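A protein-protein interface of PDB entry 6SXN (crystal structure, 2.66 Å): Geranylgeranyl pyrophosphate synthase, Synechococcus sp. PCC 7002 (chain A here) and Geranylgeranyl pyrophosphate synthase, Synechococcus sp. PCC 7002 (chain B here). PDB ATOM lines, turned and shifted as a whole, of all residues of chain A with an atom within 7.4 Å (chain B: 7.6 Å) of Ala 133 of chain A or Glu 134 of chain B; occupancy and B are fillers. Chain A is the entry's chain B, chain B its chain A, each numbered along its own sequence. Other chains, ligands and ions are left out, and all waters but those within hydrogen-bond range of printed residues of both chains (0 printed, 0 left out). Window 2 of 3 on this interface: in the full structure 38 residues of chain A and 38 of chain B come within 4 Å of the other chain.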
ATOM      1  N   ALA A 126     -12.208 -31.273  22.393  1.00  0.00           N
ATOM      2  CA  ALA A 126     -10.798 -30.938  22.464  1.00  0.00           C
ATOM      3  C   ALA A 126      -9.965 -32.191  22.699  1.00  0.00           C
ATOM      4  O   ALA A 126      -8.776 -32.168  22.412  1.00  0.00           O
ATOM      5  CB  ALA A 126     -10.596 -29.893  23.522  1.00  0.00           C
ATOM      6  N   ASP A 130      -7.394 -38.060  16.781  1.00  0.00           N
ATOM      7  CA  ASP A 130      -6.375 -38.076  15.731  1.00  0.00           C
ATOM      8  C   ASP A 130      -6.572 -36.959  14.712  1.00  0.00           C
ATOM      9  O   ASP A 130      -6.624 -37.188  13.500  1.00  0.00           O
ATOM     10  CB  ASP A 130      -6.295 -39.443  15.051  1.00  0.00           C
ATOM     11  CG  ASP A 130      -4.998 -40.173  15.311  1.00  0.00           C
ATOM     12  OD1 ASP A 130      -4.007 -39.492  15.644  1.00  0.00           O
ATOM     13  OD2 ASP A 130      -4.990 -41.403  15.139  1.00  0.00           O
ATOM     14  N   VAL A 131      -6.714 -35.744  15.213  1.00  0.00           N
ATOM     15  CA  VAL A 131      -7.097 -34.632  14.361  1.00  0.00           C
ATOM     16  C   VAL A 131      -6.155 -33.483  14.690  1.00  0.00           C
ATOM     17  O   VAL A 131      -5.915 -33.192  15.858  1.00  0.00           O
ATOM     18  CB  VAL A 131      -8.582 -34.257  14.582  1.00  0.00           C
ATOM     19  CG1 VAL A 131      -9.022 -33.086  13.739  1.00  0.00           C
ATOM     20  CG2 VAL A 131      -9.518 -35.424  14.352  1.00  0.00           C
ATOM     21  N   PRO A 132      -5.589 -32.778  13.691  1.00  0.00           N
ATOM     22  CA  PRO A 132      -4.776 -31.593  13.971  1.00  0.00           C
ATOM     23  C   PRO A 132      -5.559 -30.631  14.868  1.00  0.00           C
ATOM     24  O   PRO A 132      -6.744 -30.388  14.653  1.00  0.00           O
ATOM     25  CB  PRO A 132      -4.587 -30.911  12.596  1.00  0.00           C
ATOM     26  CG  PRO A 132      -5.071 -31.912  11.532  1.00  0.00           C
ATOM     27  CD  PRO A 132      -5.759 -33.048  12.249  1.00  0.00           C
ATOM     28  N   ALA A 133      -4.858 -30.057  15.844  1.00  0.00           N
ATOM     29  CA  ALA A 133      -5.431 -29.157  16.836  1.00  0.00           C
ATOM     30  C   ALA A 133      -6.086 -27.936  16.189  1.00  0.00           C
ATOM     31  O   ALA A 133      -7.074 -27.418  16.705  1.00  0.00           O
ATOM     32  CB  ALA A 133      -4.389 -28.762  17.850  1.00  0.00           C
ATOM     33  N   GLU A 134      -5.543 -27.468  15.068  1.00  0.00           N
ATOM     34  CA  GLU A 134      -6.046 -26.265  14.413  1.00  0.00           C
ATOM     35  C   GLU A 134      -7.499 -26.485  14.009  1.00  0.00           C
ATOM     36  O   GLU A 134      -8.323 -25.577  14.137  1.00  0.00           O
ATOM     37  CB  GLU A 134      -5.216 -25.939  13.178  1.00  0.00           C
ATOM     38  CG  GLU A 134      -3.727 -26.193  13.363  1.00  0.00           C
ATOM     39  CD  GLU A 134      -2.860 -24.981  13.689  1.00  0.00           C
ATOM     40  OE1 GLU A 134      -3.398 -23.838  13.733  1.00  0.00           O
ATOM     41  OE2 GLU A 134      -1.643 -25.192  13.921  1.00  0.00           O
ATOM     42  N   ARG A 135      -7.816 -27.710  13.563  1.00  0.00           N
ATOM     43  CA  ARG A 135      -9.180 -28.012  13.146  1.00  0.00           C
ATOM     44  C   ARG A 135     -10.094 -28.000  14.366  1.00  0.00           C
ATOM     45  O   ARG A 135     -11.162 -27.388  14.344  1.00  0.00           O
ATOM     46  CB  ARG A 135      -9.284 -29.368  12.441  1.00  0.00           C
ATOM     47  CG  ARG A 135      -8.135 -29.685  11.495  1.00  0.00           C
ATOM     48  CD  ARG A 135      -8.566 -29.637  10.042  1.00  0.00           C
ATOM     49  NE  ARG A 135      -7.693 -30.416   9.162  1.00  0.00           N
ATOM     50  CZ  ARG A 135      -7.747 -31.733   9.004  1.00  0.00           C
ATOM     51  NH1 ARG A 135      -8.621 -32.461   9.679  1.00  0.00           N
ATOM     52  NH2 ARG A 135      -6.924 -32.323   8.161  1.00  0.00           N
ATOM     53  N   LEU A 136      -9.654 -28.669  15.432  1.00  0.00           N
ATOM     54  CA  LEU A 136     -10.434 -28.746  16.651  1.00  0.00           C
ATOM     55  C   LEU A 136     -10.750 -27.344  17.186  1.00  0.00           C
ATOM     56  O   LEU A 136     -11.877 -27.107  17.645  1.00  0.00           O
ATOM     57  CB  LEU A 136      -9.693 -29.590  17.684  1.00  0.00           C
ATOM     58  CG  LEU A 136      -9.486 -31.048  17.308  1.00  0.00           C
ATOM     59  CD1 LEU A 136      -8.709 -31.800  18.380  1.00  0.00           C
ATOM     60  CD2 LEU A 136     -10.834 -31.704  17.023  1.00  0.00           C
ATOM     61  N   LEU A 137      -9.778 -26.411  17.118  1.00  0.00           N
ATOM     62  CA  LEU A 137     -10.034 -25.065  17.602  1.00  0.00           C
ATOM     63  C   LEU A 137     -11.137 -24.407  16.771  1.00  0.00           C
ATOM     64  O   LEU A 137     -11.994 -23.711  17.317  1.00  0.00           O
ATOM     65  CB  LEU A 137      -8.772 -24.216  17.558  1.00  0.00           C
ATOM     66  CG  LEU A 137      -7.796 -24.376  18.716  1.00  0.00           C
ATOM     67  CD1 LEU A 137      -6.869 -23.180  18.763  1.00  0.00           C
ATOM     68  CD2 LEU A 137      -8.551 -24.473  20.015  1.00  0.00           C
ATOM     69  N   GLN A 138     -11.097 -24.606  15.450  1.00  0.00           N
ATOM     70  CA  GLN A 138     -12.120 -24.019  14.602  1.00  0.00           C
ATOM     71  C   GLN A 138     -13.493 -24.572  14.985  1.00  0.00           C
ATOM     72  O   GLN A 138     -14.470 -23.834  15.072  1.00  0.00           O
ATOM     73  CB  GLN A 138     -11.815 -24.259  13.133  1.00  0.00           C
ATOM     74  CG  GLN A 138     -10.638 -23.456  12.615  1.00  0.00           C
ATOM     75  CD  GLN A 138     -10.526 -23.683  11.120  1.00  0.00           C
ATOM     76  OE1 GLN A 138      -9.904 -24.647  10.640  1.00  0.00           O
ATOM     77  NE2 GLN A 138     -11.180 -22.808  10.367  1.00  0.00           N
ATOM     78  N   VAL A 139     -13.563 -25.880  15.253  1.00  0.00           N
ATOM     79  CA  VAL A 139     -14.833 -26.476  15.634  1.00  0.00           C
ATOM     80  C   VAL A 139     -15.302 -25.799  16.920  1.00  0.00           C
ATOM     81  O   VAL A 139     -16.457 -25.415  17.015  1.00  0.00           O
ATOM     82  CB  VAL A 139     -14.728 -28.000  15.799  1.00  0.00           C
ATOM     83  CG1 VAL A 139     -15.990 -28.603  16.408  1.00  0.00           C
ATOM     84  CG2 VAL A 139     -14.388 -28.668  14.505  1.00  0.00           C
ATOM     85  N   ILE A 140     -14.374 -25.647  17.885  1.00  0.00           N
ATOM     86  CA  ILE A 140     -14.693 -25.093  19.188  1.00  0.00           C
ATOM     87  C   ILE A 140     -15.212 -23.664  19.026  1.00  0.00           C
ATOM     88  O   ILE A 140     -16.198 -23.280  19.661  1.00  0.00           O
ATOM     89  CB  ILE A 140     -13.500 -25.220  20.149  1.00  0.00           C
ATOM     90  CG1 ILE A 140     -13.372 -26.667  20.618  1.00  0.00           C
ATOM     91  CG2 ILE A 140     -13.642 -24.262  21.335  1.00  0.00           C
ATOM     92  CD1 ILE A 140     -12.106 -26.961  21.380  1.00  0.00           C
ATOM     93  N   VAL B 131      -0.912 -18.037  19.638  1.00  0.00           N
ATOM     94  CA  VAL B 131      -0.460 -19.028  20.595  1.00  0.00           C
ATOM     95  C   VAL B 131      -0.611 -20.383  19.919  1.00  0.00           C
ATOM     96  O   VAL B 131      -1.642 -20.639  19.293  1.00  0.00           O
ATOM     97  CB  VAL B 131      -1.270 -18.946  21.912  1.00  0.00           C
ATOM     98  CG1 VAL B 131      -0.962 -20.072  22.911  1.00  0.00           C
ATOM     99  CG2 VAL B 131      -1.164 -17.566  22.564  1.00  0.00           C
ATOM    100  N   PRO B 132       0.398 -21.278  19.999  1.00  0.00           N
ATOM    101  CA  PRO B 132       0.288 -22.586  19.367  1.00  0.00           C
ATOM    102  C   PRO B 132      -0.999 -23.281  19.812  1.00  0.00           C
ATOM    103  O   PRO B 132      -1.348 -23.241  21.000  1.00  0.00           O
ATOM    104  CB  PRO B 132       1.488 -23.389  19.896  1.00  0.00           C
ATOM    105  CG  PRO B 132       2.411 -22.406  20.566  1.00  0.00           C
ATOM    106  CD  PRO B 132       1.671 -21.096  20.711  1.00  0.00           C
ATOM    107  N   ALA B 133      -1.683 -23.917  18.846  1.00  0.00           N
ATOM    108  CA  ALA B 133      -2.976 -24.544  19.080  1.00  0.00           C
ATOM    109  C   ALA B 133      -2.894 -25.639  20.155  1.00  0.00           C
ATOM    110  O   ALA B 133      -3.850 -25.841  20.898  1.00  0.00           O
ATOM    111  CB  ALA B 133      -3.531 -25.062  17.794  1.00  0.00           C
ATOM    112  N   GLU B 134      -1.750 -26.319  20.256  1.00  0.00           N
ATOM    113  CA  GLU B 134      -1.600 -27.418  21.192  1.00  0.00           C
ATOM    114  C   GLU B 134      -1.796 -26.903  22.609  1.00  0.00           C
ATOM    115  O   GLU B 134      -2.410 -27.574  23.444  1.00  0.00           O
ATOM    116  CB  GLU B 134      -0.215 -28.049  21.060  1.00  0.00           C
ATOM    117  CG  GLU B 134       0.110 -28.374  19.620  1.00  0.00           C
ATOM    118  CD  GLU B 134      -0.640 -29.555  18.999  1.00  0.00           C
ATOM    119  OE1 GLU B 134      -1.304 -30.323  19.765  1.00  0.00           O
ATOM    120  OE2 GLU B 134      -0.575 -29.702  17.745  1.00  0.00           O
ATOM    121  N   ARG B 135      -1.289 -25.695  22.872  1.00  0.00           N
ATOM    122  CA  ARG B 135      -1.391 -25.118  24.204  1.00  0.00           C
ATOM    123  C   ARG B 135      -2.861 -24.812  24.482  1.00  0.00           C
ATOM    124  O   ARG B 135      -3.381 -25.147  25.545  1.00  0.00           O
ATOM    125  CB  ARG B 135      -0.538 -23.838  24.343  1.00  0.00           C
ATOM    126  CG  ARG B 135       0.834 -23.914  23.690  1.00  0.00           C
ATOM    127  CD  ARG B 135       1.977 -24.042  24.682  1.00  0.00           C
ATOM    128  NE  ARG B 135       3.252 -23.573  24.139  1.00  0.00           N
ATOM    129  CZ  ARG B 135       3.624 -22.293  24.047  1.00  0.00           C
ATOM    130  NH1 ARG B 135       2.830 -21.310  24.431  1.00  0.00           N
ATOM    131  NH2 ARG B 135       4.815 -22.008  23.566  1.00  0.00           N
ATOM    132  N   LEU B 136      -3.511 -24.138  23.520  1.00  0.00           N
ATOM    133  CA  LEU B 136      -4.895 -23.744  23.669  1.00  0.00           C
ATOM    134  C   LEU B 136      -5.778 -24.963  23.959  1.00  0.00           C
ATOM    135  O   LEU B 136      -6.677 -24.859  24.806  1.00  0.00           O
ATOM    136  CB  LEU B 136      -5.341 -23.000  22.413  1.00  0.00           C
ATOM    137  CG  LEU B 136      -4.696 -21.624  22.224  1.00  0.00           C
ATOM    138  CD1 LEU B 136      -5.247 -20.932  20.982  1.00  0.00           C
ATOM    139  CD2 LEU B 136      -4.831 -20.726  23.466  1.00  0.00           C
ATOM    140  N   LEU B 137      -5.508 -26.103  23.292  1.00  0.00           N
ATOM    141  CA  LEU B 137      -6.314 -27.287  23.521  1.00  0.00           C
ATOM    142  C   LEU B 137      -6.152 -27.742  24.965  1.00  0.00           C
ATOM    143  O   LEU B 137      -7.138 -28.115  25.599  1.00  0.00           O
ATOM    144  CB  LEU B 137      -5.891 -28.426  22.594  1.00  0.00           C
ATOM    145  CG  LEU B 137      -6.443 -28.417  21.165  1.00  0.00           C
ATOM    146  CD1 LEU B 137      -6.449 -29.823  20.620  1.00  0.00           C
ATOM    147  CD2 LEU B 137      -7.838 -27.829  21.057  1.00  0.00           C
ATOM    148  N   GLN B 138      -4.907 -27.720  25.473  1.00  0.00           N
ATOM    149  CA  GLN B 138      -4.673 -28.134  26.845  1.00  0.00           C
ATOM    150  C   GLN B 138      -5.454 -27.233  27.794  1.00  0.00           C
ATOM    151  O   GLN B 138      -6.072 -27.722  28.733  1.00  0.00           O
ATOM    152  CB  GLN B 138      -3.190 -28.125  27.182  1.00  0.00           C
ATOM    153  CG  GLN B 138      -2.429 -29.253  26.502  1.00  0.00           C
ATOM    154  CD  GLN B 138      -0.958 -28.935  26.510  1.00  0.00           C
ATOM    155  OE1 GLN B 138      -0.422 -28.196  25.672  1.00  0.00           O
ATOM    156  NE2 GLN B 138      -0.323 -29.434  27.546  1.00  0.00           N
ATOM    157  N   VAL B 139      -5.447 -25.923  27.534  1.00  0.00           N
ATOM    158  CA  VAL B 139      -6.155 -25.002  28.398  1.00  0.00           C
ATOM    159  C   VAL B 139      -7.632 -25.382  28.389  1.00  0.00           C
ATOM    160  O   VAL B 139      -8.252 -25.479  29.451  1.00  0.00           O
ATOM    161  CB  VAL B 139      -5.924 -23.536  28.004  1.00  0.00           C
ATOM    162  CG1 VAL B 139      -6.817 -22.584  28.782  1.00  0.00           C
ATOM    163  CG2 VAL B 139      -4.462 -23.183  28.227  1.00  0.00           C
ATOM    164  N   ILE B 140      -8.156 -25.628  27.182  1.00  0.00           N
ATOM    165  CA  ILE B 140      -9.578 -25.907  27.018  1.00  0.00           C
ATOM    166  C   ILE B 140      -9.937 -27.195  27.758  1.00  0.00           C
ATOM    167  O   ILE B 140     -10.958 -27.252  28.437  1.00  0.00           O
ATOM    168  CB  ILE B 140      -9.953 -25.923  25.526  1.00  0.00           C
ATOM    169  CG1 ILE B 140      -9.962 -24.499  24.979  1.00  0.00           C
ATOM    170  CG2 ILE B 140     -11.282 -26.651  25.305  1.00  0.00           C
ATOM    171  CD1 ILE B 140     -10.177 -24.382  23.515  1.00  0.00           C
ATOM    172  N   ILE B 193       0.622 -22.841  31.090  1.00  0.00           N
ATOM    173  CA  ILE B 193       0.583 -23.571  29.830  1.00  0.00           C
ATOM    174  C   ILE B 193       0.662 -22.597  28.660  1.00  0.00           C
ATOM    175  O   ILE B 193       1.406 -22.810  27.715  1.00  0.00           O
ATOM    176  CB  ILE B 193      -0.649 -24.510  29.759  1.00  0.00           C
ATOM    177  CG1 ILE B 193      -0.464 -25.716  30.694  1.00  0.00           C
ATOM    178  CG2 ILE B 193      -0.946 -24.953  28.311  1.00  0.00           C
ATOM    179  CD1 ILE B 193      -1.762 -26.229  31.224  1.00  0.00           C
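The side-chain amide oxygen (OE1) of Gln 138 of chain B lies close to the backbone carbonyl oxygen (O) of Glu 134 of chain B, at 3.1 Å.
CD1 of Leu 137 of chain B touches O of Ala 126 of chain A, 3.8 Å away.
Ile 140 of chain B touches Ala 126 of chain A (CG2 to CB, 3.8 Å).
Ala 133 of chain A touches Glu 134 of chain B (CB to OE2, 3.9 Å).
Leu 137 of chain B touches Ala 133 of chain A (CD1 to CB, 3.6 Å).
Leu 137 of chain B touches Leu 136 of chain A (CD1 to CD1, 3.7 Å).
CD1 of Leu 137 of chain A touches CB of Ala 133 of chain B, at 3.95 Å.
Leu 136 of chain B touches Leu 137 of chain A (CD1 to CD1, 3.6 Å).
CD2 of Leu 137 of chain A touches CD2 of Leu 137 of chain B (3.6 Å).
Ile 140 of chain B touches Leu 137 of chain A (CD1 to CD2, 3.9 Å).
Ile 140 of chain A touches Ile 140 of chain B (CD1 to CD1, 3.9 Å).
Printed residues of chain B within 4 Å of Ala 126 of chain A: Leu 137 and Ile 140.
Val 139 of chain A touches none of the printed residues of chain B.
Of the printed residues of chain B, Ile 140 of chain A touches Ile 140 (3.9 Å).
Ala 133 of chain B touches just these residues of chain A: Ala 133 (3.8 Å) and Leu 137 (3.95 Å).
Glu 134 of chain B touches just one residue of chain A: Ala 133.
Printed residues of chain A within 4 Å of Leu 137 of chain B: Ala 126, Ala 133, Leu 136 and Leu 137.
Among the printed residues, no Asp or Glu carboxylate lies within 4 Å of a Lys or Arg side-chain nitrogen of the other chain.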
